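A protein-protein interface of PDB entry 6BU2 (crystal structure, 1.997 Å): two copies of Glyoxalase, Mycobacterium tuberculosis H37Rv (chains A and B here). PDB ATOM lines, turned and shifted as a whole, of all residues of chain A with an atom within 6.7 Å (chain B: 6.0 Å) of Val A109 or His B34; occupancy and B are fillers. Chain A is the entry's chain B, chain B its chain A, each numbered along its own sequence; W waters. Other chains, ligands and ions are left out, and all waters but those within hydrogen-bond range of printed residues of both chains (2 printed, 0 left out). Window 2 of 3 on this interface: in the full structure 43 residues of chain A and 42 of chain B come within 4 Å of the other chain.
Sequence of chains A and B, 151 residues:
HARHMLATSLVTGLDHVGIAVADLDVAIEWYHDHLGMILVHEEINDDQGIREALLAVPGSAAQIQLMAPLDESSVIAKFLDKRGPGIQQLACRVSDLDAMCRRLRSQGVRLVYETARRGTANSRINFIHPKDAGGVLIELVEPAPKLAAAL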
ATOM      1  N   SER A   9      18.834  -2.248 -14.951  1.00  0.00           N
ATOM      2  CA  SER A   9      18.662  -2.967 -16.205  1.00  0.00           C
ATOM      3  C   SER A   9      20.033  -3.244 -16.809  1.00  0.00           C
ATOM      4  O   SER A   9      21.075  -2.956 -16.218  1.00  0.00           O
ATOM      5  CB  SER A   9      17.789  -2.174 -17.175  1.00  0.00           C
ATOM      6  OG  SER A   9      18.454  -0.996 -17.608  1.00  0.00           O
ATOM      7  N   VAL A  11      20.952  -1.772 -19.485  1.00  0.00           N
ATOM      8  CA  VAL A  11      21.311  -0.533 -20.169  1.00  0.00           C
ATOM      9  C   VAL A  11      22.448   0.129 -19.402  1.00  0.00           C
ATOM     10  O   VAL A  11      22.331   0.394 -18.200  1.00  0.00           O
ATOM     11  CB  VAL A  11      20.100   0.403 -20.278  1.00  0.00           C
ATOM     12  CG1 VAL A  11      20.499   1.819 -20.847  1.00  0.00           C
ATOM     13  CG2 VAL A  11      18.999  -0.257 -21.115  1.00  0.00           C
ATOM     14  N   MET A 100      19.312  -8.966 -22.384  1.00  0.00           N
ATOM     15  CA  MET A 100      18.304  -7.907 -22.434  1.00  0.00           C
ATOM     16  C   MET A 100      17.086  -8.336 -23.237  1.00  0.00           C
ATOM     17  O   MET A 100      15.941  -8.095 -22.830  1.00  0.00           O
ATOM     18  CB  MET A 100      18.881  -6.633 -23.053  1.00  0.00           C
ATOM     19  CG  MET A 100      17.859  -5.464 -23.090  1.00  0.00           C
ATOM     20  SD  MET A 100      18.274  -4.028 -22.105  1.00  0.00           S
ATOM     21  CE  MET A 100      16.773  -3.060 -22.156  1.00  0.00           C
ATOM     22  N   CYS A 101      17.310  -8.941 -24.401  1.00  0.00           N
ATOM     23  CA  CYS A 101      16.196  -9.295 -25.271  1.00  0.00           C
ATOM     24  C   CYS A 101      15.312 -10.355 -24.627  1.00  0.00           C
ATOM     25  O   CYS A 101      14.080 -10.245 -24.659  1.00  0.00           O
ATOM     26  CB  CYS A 101      16.723  -9.749 -26.636  1.00  0.00           C
ATOM     27  SG  CYS A 101      17.386  -8.346 -27.610  1.00  0.00           S
ATOM     28  N   ARG A 103      14.928 -10.833 -21.440  1.00  0.00           N
ATOM     29  CA  ARG A 103      14.193 -10.146 -20.377  1.00  0.00           C
ATOM     30  C   ARG A 103      13.011  -9.370 -20.951  1.00  0.00           C
ATOM     31  O   ARG A 103      11.891  -9.443 -20.432  1.00  0.00           O
ATOM     32  CB  ARG A 103      15.116  -9.202 -19.596  1.00  0.00           C
ATOM     33  CG  ARG A 103      16.210  -9.870 -18.758  1.00  0.00           C
ATOM     34  CD  ARG A 103      16.390  -9.164 -17.398  1.00  0.00           C
ATOM     35  NE  ARG A 103      17.795  -8.973 -17.022  1.00  0.00           N
ATOM     36  CZ  ARG A 103      18.561  -9.904 -16.453  1.00  0.00           C
ATOM     37  NH1 ARG A 103      19.823  -9.633 -16.145  1.00  0.00           N
ATOM     38  NH2 ARG A 103      18.075 -11.111 -16.195  1.00  0.00           N
ATOM     39  N   LEU A 104      13.251  -8.611 -22.020  1.00  0.00           N
ATOM     40  CA  LEU A 104      12.180  -7.850 -22.661  1.00  0.00           C
ATOM     41  C   LEU A 104      11.050  -8.755 -23.149  1.00  0.00           C
ATOM     42  O   LEU A 104       9.869  -8.424 -22.981  1.00  0.00           O
ATOM     43  CB  LEU A 104      12.756  -7.027 -23.812  1.00  0.00           C
ATOM     44  CG  LEU A 104      13.596  -5.835 -23.320  1.00  0.00           C
ATOM     45  CD1 LEU A 104      14.394  -5.252 -24.434  1.00  0.00           C
ATOM     46  CD2 LEU A 104      12.681  -4.765 -22.737  1.00  0.00           C
ATOM     47  N   ARG A 105      11.388  -9.897 -23.759  1.00  0.00           N
ATOM     48  CA  ARG A 105      10.348 -10.792 -24.264  1.00  0.00           C
ATOM     49  C   ARG A 105       9.545 -11.420 -23.134  1.00  0.00           C
ATOM     50  O   ARG A 105       8.323 -11.574 -23.250  1.00  0.00           O
ATOM     51  CB  ARG A 105      10.959 -11.877 -25.152  1.00  0.00           C
ATOM     52  CG  ARG A 105      11.297 -11.368 -26.546  1.00  0.00           C
ATOM     53  CD  ARG A 105      11.596 -12.499 -27.478  1.00  0.00           C
ATOM     54  NE  ARG A 105      11.795 -12.013 -28.842  1.00  0.00           N
ATOM     55  CZ  ARG A 105      12.983 -11.877 -29.421  1.00  0.00           C
ATOM     56  NH1 ARG A 105      13.070 -11.450 -30.679  1.00  0.00           N
ATOM     57  NH2 ARG A 105      14.076 -12.170 -28.732  1.00  0.00           N
ATOM     58  N   SER A 106      10.206 -11.783 -22.032  1.00  0.00           N
ATOM     59  CA  SER A 106       9.468 -12.325 -20.898  1.00  0.00           C
ATOM     60  C   SER A 106       8.672 -11.243 -20.173  1.00  0.00           C
ATOM     61  O   SER A 106       7.755 -11.573 -19.412  1.00  0.00           O
ATOM     62  CB  SER A 106      10.417 -13.043 -19.933  1.00  0.00           C
ATOM     63  OG  SER A 106      11.070 -12.126 -19.072  1.00  0.00           O
ATOM     64  N   GLN A 107       8.990  -9.963 -20.399  1.00  0.00           N
ATOM     65  CA  GLN A 107       8.182  -8.856 -19.895  1.00  0.00           C
ATOM     66  C   GLN A 107       7.044  -8.481 -20.834  1.00  0.00           C
ATOM     67  O   GLN A 107       6.328  -7.509 -20.560  1.00  0.00           O
ATOM     68  CB  GLN A 107       9.050  -7.613 -19.653  1.00  0.00           C
ATOM     69  CG  GLN A 107      10.005  -7.710 -18.476  1.00  0.00           C
ATOM     70  CD  GLN A 107      11.119  -6.670 -18.542  1.00  0.00           C
ATOM     71  OE1 GLN A 107      11.089  -5.747 -19.375  1.00  0.00           O
ATOM     72  NE2 GLN A 107      12.112  -6.818 -17.670  1.00  0.00           N
ATOM     73  N   GLY A 108       6.872  -9.202 -21.939  1.00  0.00           N
ATOM     74  CA  GLY A 108       5.803  -8.905 -22.869  1.00  0.00           C
ATOM     75  C   GLY A 108       6.107  -7.851 -23.909  1.00  0.00           C
ATOM     76  O   GLY A 108       5.169  -7.310 -24.504  1.00  0.00           O
ATOM     77  N   VAL A 109       7.382  -7.528 -24.140  1.00  0.00           N
ATOM     78  CA  VAL A 109       7.796  -6.556 -25.158  1.00  0.00           C
ATOM     79  C   VAL A 109       8.448  -7.307 -26.308  1.00  0.00           C
ATOM     80  O   VAL A 109       9.305  -8.173 -26.087  1.00  0.00           O
ATOM     81  CB  VAL A 109       8.752  -5.494 -24.586  1.00  0.00           C
ATOM     82  CG1 VAL A 109       9.373  -4.661 -25.705  1.00  0.00           C
ATOM     83  CG2 VAL A 109       8.014  -4.585 -23.624  1.00  0.00           C
ATOM     84  N   ARG A 110       8.024  -6.999 -27.527  1.00  0.00           N
ATOM     85  CA  ARG A 110       8.522  -7.641 -28.732  1.00  0.00           C
ATOM     86  C   ARG A 110       9.803  -6.975 -29.229  1.00  0.00           C
ATOM     87  O   ARG A 110      10.013  -5.765 -29.058  1.00  0.00           O
ATOM     88  CB  ARG A 110       7.464  -7.598 -29.841  1.00  0.00           C
ATOM     89  CG  ARG A 110       6.311  -8.601 -29.693  1.00  0.00           C
ATOM     90  CD  ARG A 110       5.291  -8.454 -30.846  1.00  0.00           C
ATOM     91  NE  ARG A 110       4.693  -7.118 -30.873  1.00  0.00           N
ATOM     92  CZ  ARG A 110       4.100  -6.569 -31.934  1.00  0.00           C
ATOM     93  NH1 ARG A 110       4.007  -7.233 -33.080  1.00  0.00           N
ATOM     94  NH2 ARG A 110       3.596  -5.345 -31.846  1.00  0.00           N
ATOM     95  N   LEU A 111      10.654  -7.781 -29.863  1.00  0.00           N
ATOM     96  CA  LEU A 111      11.845  -7.302 -30.545  1.00  0.00           C
ATOM     97  C   LEU A 111      11.676  -7.508 -32.047  1.00  0.00           C
ATOM     98  O   LEU A 111      10.980  -8.419 -32.491  1.00  0.00           O
ATOM     99  CB  LEU A 111      13.107  -8.029 -30.049  1.00  0.00           C
ATOM    100  CG  LEU A 111      13.692  -7.639 -28.679  1.00  0.00           C
ATOM    101  CD1 LEU A 111      14.032  -6.142 -28.622  1.00  0.00           C
ATOM    102  CD2 LEU A 111      12.804  -8.038 -27.488  1.00  0.00           C
ATOM    103  N   ILE A 128      13.499  -2.701 -30.139  1.00  0.00           N
ATOM    104  CA  ILE A 128      12.169  -2.910 -29.588  1.00  0.00           C
ATOM    105  C   ILE A 128      11.161  -2.616 -30.683  1.00  0.00           C
ATOM    106  O   ILE A 128      11.326  -1.678 -31.474  1.00  0.00           O
ATOM    107  CB  ILE A 128      11.938  -2.035 -28.346  1.00  0.00           C
ATOM    108  CG1 ILE A 128      12.840  -2.510 -27.211  1.00  0.00           C
ATOM    109  CG2 ILE A 128      10.491  -2.109 -27.894  1.00  0.00           C
ATOM    110  CD1 ILE A 128      12.770  -1.636 -25.975  1.00  0.00           C
ATOM    111  N   HIS A 129      10.144  -3.451 -30.786  1.00  0.00           N
ATOM    112  CA  HIS A 129       9.148  -3.228 -31.818  1.00  0.00           C
ATOM    113  C   HIS A 129       8.536  -1.845 -31.618  1.00  0.00           C
ATOM    114  O   HIS A 129       8.069  -1.531 -30.514  1.00  0.00           O
ATOM    115  CB  HIS A 129       8.075  -4.320 -31.784  1.00  0.00           C
ATOM    116  CG  HIS A 129       7.236  -4.377 -33.020  1.00  0.00           C
ATOM    117  ND1 HIS A 129       6.532  -3.287 -33.494  1.00  0.00           N
ATOM    118  CD2 HIS A 129       6.987  -5.392 -33.883  1.00  0.00           C
ATOM    119  CE1 HIS A 129       5.877  -3.633 -34.587  1.00  0.00           C
ATOM    120  NE2 HIS A 129       6.138  -4.903 -34.846  1.00  0.00           N
ATOM    121  N   ASP A 132       5.212  -1.476 -30.000  1.00  0.00           N
ATOM    122  CA  ASP A 132       5.243  -1.738 -28.567  1.00  0.00           C
ATOM    123  C   ASP A 132       5.740  -0.547 -27.762  1.00  0.00           C
ATOM    124  O   ASP A 132       5.453  -0.472 -26.565  1.00  0.00           O
ATOM    125  CB  ASP A 132       6.124  -2.950 -28.269  1.00  0.00           C
ATOM    126  CG  ASP A 132       5.512  -4.233 -28.749  1.00  0.00           C
ATOM    127  OD1 ASP A 132       4.843  -4.210 -29.797  1.00  0.00           O
ATOM    128  OD2 ASP A 132       5.682  -5.256 -28.071  1.00  0.00           O
ATOM    129  N   ALA A 133       6.500   0.363 -28.378  1.00  0.00           N
ATOM    130  CA  ALA A 133       7.038   1.536 -27.698  1.00  0.00           C
ATOM    131  C   ALA A 133       6.314   2.815 -28.102  1.00  0.00           C
ATOM    132  O   ALA A 133       6.910   3.905 -28.096  1.00  0.00           O
ATOM    133  CB  ALA A 133       8.537   1.663 -27.966  1.00  0.00           C
ATOM    134  N   GLU B  29       6.315   4.840 -16.524  1.00  0.00           N
ATOM    135  CA  GLU B  29       6.425   3.499 -15.964  1.00  0.00           C
ATOM    136  C   GLU B  29       7.003   2.521 -16.982  1.00  0.00           C
ATOM    137  O   GLU B  29       7.769   1.621 -16.622  1.00  0.00           O
ATOM    138  CB  GLU B  29       5.058   3.023 -15.478  1.00  0.00           C
ATOM    139  CG  GLU B  29       4.858   3.217 -13.988  1.00  0.00           C
ATOM    140  CD  GLU B  29       3.580   2.583 -13.486  1.00  0.00           C
ATOM    141  OE1 GLU B  29       2.579   3.317 -13.323  1.00  0.00           O
ATOM    142  OE2 GLU B  29       3.566   1.349 -13.273  1.00  0.00           O
ATOM    143  N   TRP B  30       6.640   2.686 -18.255  1.00  0.00           N
ATOM    144  CA  TRP B  30       7.110   1.774 -19.292  1.00  0.00           C
ATOM    145  C   TRP B  30       8.618   1.895 -19.492  1.00  0.00           C
ATOM    146  O   TRP B  30       9.331   0.883 -19.539  1.00  0.00           O
ATOM    147  CB  TRP B  30       6.364   2.055 -20.596  1.00  0.00           C
ATOM    148  CG  TRP B  30       6.573   1.023 -21.673  1.00  0.00           C
ATOM    149  CD1 TRP B  30       5.758  -0.049 -21.961  1.00  0.00           C
ATOM    150  CD2 TRP B  30       7.651   0.969 -22.617  1.00  0.00           C
ATOM    151  NE1 TRP B  30       6.272  -0.761 -23.018  1.00  0.00           N
ATOM    152  CE2 TRP B  30       7.436  -0.164 -23.435  1.00  0.00           C
ATOM    153  CE3 TRP B  30       8.785   1.758 -22.841  1.00  0.00           C
ATOM    154  CZ2 TRP B  30       8.310  -0.520 -24.457  1.00  0.00           C
ATOM    155  CZ3 TRP B  30       9.648   1.403 -23.853  1.00  0.00           C
ATOM    156  CH2 TRP B  30       9.405   0.279 -24.655  1.00  0.00           C
ATOM    157  N   TYR B  31       9.120   3.133 -19.628  1.00  0.00           N
ATOM    158  CA  TYR B  31      10.564   3.357 -19.692  1.00  0.00           C
ATOM    159  C   TYR B  31      11.261   2.875 -18.428  1.00  0.00           C
ATOM    160  O   TYR B  31      12.384   2.354 -18.498  1.00  0.00           O
ATOM    161  CB  TYR B  31      10.868   4.849 -19.946  1.00  0.00           C
ATOM    162  CG  TYR B  31      10.703   5.219 -21.389  1.00  0.00           C
ATOM    163  CD1 TYR B  31       9.440   5.416 -21.933  1.00  0.00           C
ATOM    164  CD2 TYR B  31      11.807   5.314 -22.229  1.00  0.00           C
ATOM    165  CE1 TYR B  31       9.285   5.723 -23.294  1.00  0.00           C
ATOM    166  CE2 TYR B  31      11.659   5.644 -23.586  1.00  0.00           C
ATOM    167  CZ  TYR B  31      10.398   5.837 -24.098  1.00  0.00           C
ATOM    168  OH  TYR B  31      10.274   6.148 -25.427  1.00  0.00           O
ATOM    169  N   HIS B  32      10.619   3.016 -17.265  1.00  0.00           N
ATOM    170  CA  HIS B  32      11.264   2.520 -16.057  1.00  0.00           C
ATOM    171  C   HIS B  32      11.280   0.992 -16.028  1.00  0.00           C
ATOM    172  O   HIS B  32      12.326   0.376 -15.789  1.00  0.00           O
ATOM    173  CB  HIS B  32      10.583   3.066 -14.799  1.00  0.00           C
ATOM    174  CG  HIS B  32      11.055   2.395 -13.555  1.00  0.00           C
ATOM    175  ND1 HIS B  32      12.335   2.543 -13.075  1.00  0.00           N
ATOM    176  CD2 HIS B  32      10.455   1.499 -12.740  1.00  0.00           C
ATOM    177  CE1 HIS B  32      12.494   1.798 -11.996  1.00  0.00           C
ATOM    178  NE2 HIS B  32      11.367   1.147 -11.773  1.00  0.00           N
ATOM    179  N   ASP B  33      10.122   0.364 -16.257  1.00  0.00           N
ATOM    180  CA  ASP B  33      10.028  -1.088 -16.137  1.00  0.00           C
ATOM    181  C   ASP B  33      10.962  -1.781 -17.113  1.00  0.00           C
ATOM    182  O   ASP B  33      11.687  -2.707 -16.739  1.00  0.00           O
ATOM    183  CB  ASP B  33       8.590  -1.547 -16.373  1.00  0.00           C
ATOM    184  CG  ASP B  33       7.670  -1.137 -15.253  1.00  0.00           C
ATOM    185  OD1 ASP B  33       6.434  -1.247 -15.413  1.00  0.00           O
ATOM    186  OD2 ASP B  33       8.194  -0.688 -14.213  1.00  0.00           O
ATOM    187  N   HIS B  34      10.970  -1.334 -18.367  1.00  0.00           N
ATOM    188  CA  HIS B  34      11.605  -2.091 -19.433  1.00  0.00           C
ATOM    189  C   HIS B  34      13.024  -1.647 -19.745  1.00  0.00           C
ATOM    190  O   HIS B  34      13.795  -2.440 -20.295  1.00  0.00           O
ATOM    191  CB  HIS B  34      10.748  -2.010 -20.702  1.00  0.00           C
ATOM    192  CG  HIS B  34       9.359  -2.526 -20.509  1.00  0.00           C
ATOM    193  ND1 HIS B  34       9.099  -3.795 -20.028  1.00  0.00           N
ATOM    194  CD2 HIS B  34       8.153  -1.941 -20.696  1.00  0.00           C
ATOM    195  CE1 HIS B  34       7.793  -3.972 -19.940  1.00  0.00           C
ATOM    196  NE2 HIS B  34       7.195  -2.861 -20.333  1.00  0.00           N
ATOM    197  N   LEU B  35      13.396  -0.403 -19.430  1.00  0.00           N
ATOM    198  CA  LEU B  35      14.752   0.063 -19.706  1.00  0.00           C
ATOM    199  C   LEU B  35      15.510   0.448 -18.444  1.00  0.00           C
ATOM    200  O   LEU B  35      16.693   0.799 -18.530  1.00  0.00           O
ATOM    201  CB  LEU B  35      14.738   1.250 -20.683  1.00  0.00           C
ATOM    202  CG  LEU B  35      14.068   1.035 -22.050  1.00  0.00           C
ATOM    203  CD1 LEU B  35      14.011   2.334 -22.835  1.00  0.00           C
ATOM    204  CD2 LEU B  35      14.778  -0.014 -22.873  1.00  0.00           C
ATOM    205  N   GLY B  36      14.876   0.376 -17.280  1.00  0.00           N
ATOM    206  CA  GLY B  36      15.555   0.705 -16.048  1.00  0.00           C
ATOM    207  C   GLY B  36      15.831   2.179 -15.856  1.00  0.00           C
ATOM    208  O   GLY B  36      16.650   2.543 -15.009  1.00  0.00           O
HETATM  209  O   HOH W   1      19.032   1.156 -14.941  1.00  0.00           O
HETATM  210  O   HOH W   2       7.952   5.789 -26.523  1.00  0.00           O
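No position is printed for both chains. Of the 10 pairs that touch across the chains among the printed residues, none has its exchanged pair printed and touching as well.
Water W2 bridges OH of Tyr B31 (2.6 Å) and O of Ala A133 (2.7 Å). Water W1 bridges O of Gly B36 (2.8 Å) and N of Ser A9 (3.4 Å).
The backbone carbonyl oxygen (O) of Tyr B31 lies within hydrogen-bond range of the backbone NH (N) of Gly B36. N of Val A11 lies close to OG of Ser A9. The backbone NH of Val A109 sits at hydrogen-bond distance from the backbone carbonyl oxygen of Leu A104. The side-chain carboxylate (OD1) of Asp A132 lies within salt-bridge range of the guanidinium group (NH2) of Arg A110, at 2.7 Å.
The side-chain amide oxygen (OE1) of Gln A107 is in hydrogen-bond range of a ring nitrogen (ND1) of His B34. The backbone carbonyl oxygen (O) of Leu B35 sits at hydrogen-bond distance from the side-chain hydroxyl (OG) of Ser A9 (2.7 Å).
Of the printed residues of chain B, Ser A9 touches Leu B35 (2.7 Å) and Gly B36 (3.7 Å). Printed residues of chain B within 4 Å of Leu A104: His B34 (3.6 Å). Of chain B, only His B34 comes within 4 Å of Val A109. Printed residues of chain B within 4 Å of Ala A133: Trp B30. Of the printed residues of chain A, Trp B30 touches Asp A132 and Ala A133. Tyr B31 touches none of the printed residues of chain A. Printed residues of chain A within 4 Å of His B34: Met A100, Leu A104, Gln A107 and Val A109. The nearest residue of chain A that does not touch His B34 is Ser A9 (5.1 Å). The nearest printed residue of chain B that does not touch Ser A9 is His B34 (5.1 Å).
Printed residues of chain A that touch a printed residue of chain B: Ser A9, Val A11, Met A100, Leu A104, Gln A107, Val A109, Asp A132 and Ala A133. Hydrophobic or aromatic side chains of chain A within 4 Å of the printed part of chain B: Val A11, Met A100, Leu A104, Val A109 and Ala A133. Among the printed residues, no Asp or Glu carboxylate lies within 4 Å of a Lys or Arg side-chain nitrogen of the other chain.
Among the printed residues, pairs that only touch across the chains: Asp A132 with Trp B30, Leu A104 with His B34, Met A100 with His B34, Val A11 with Leu B35, Ala A133 with Trp B30, Ser A9 with Gly B36, Met A100 with Leu B35 and Val A109 with His B34.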
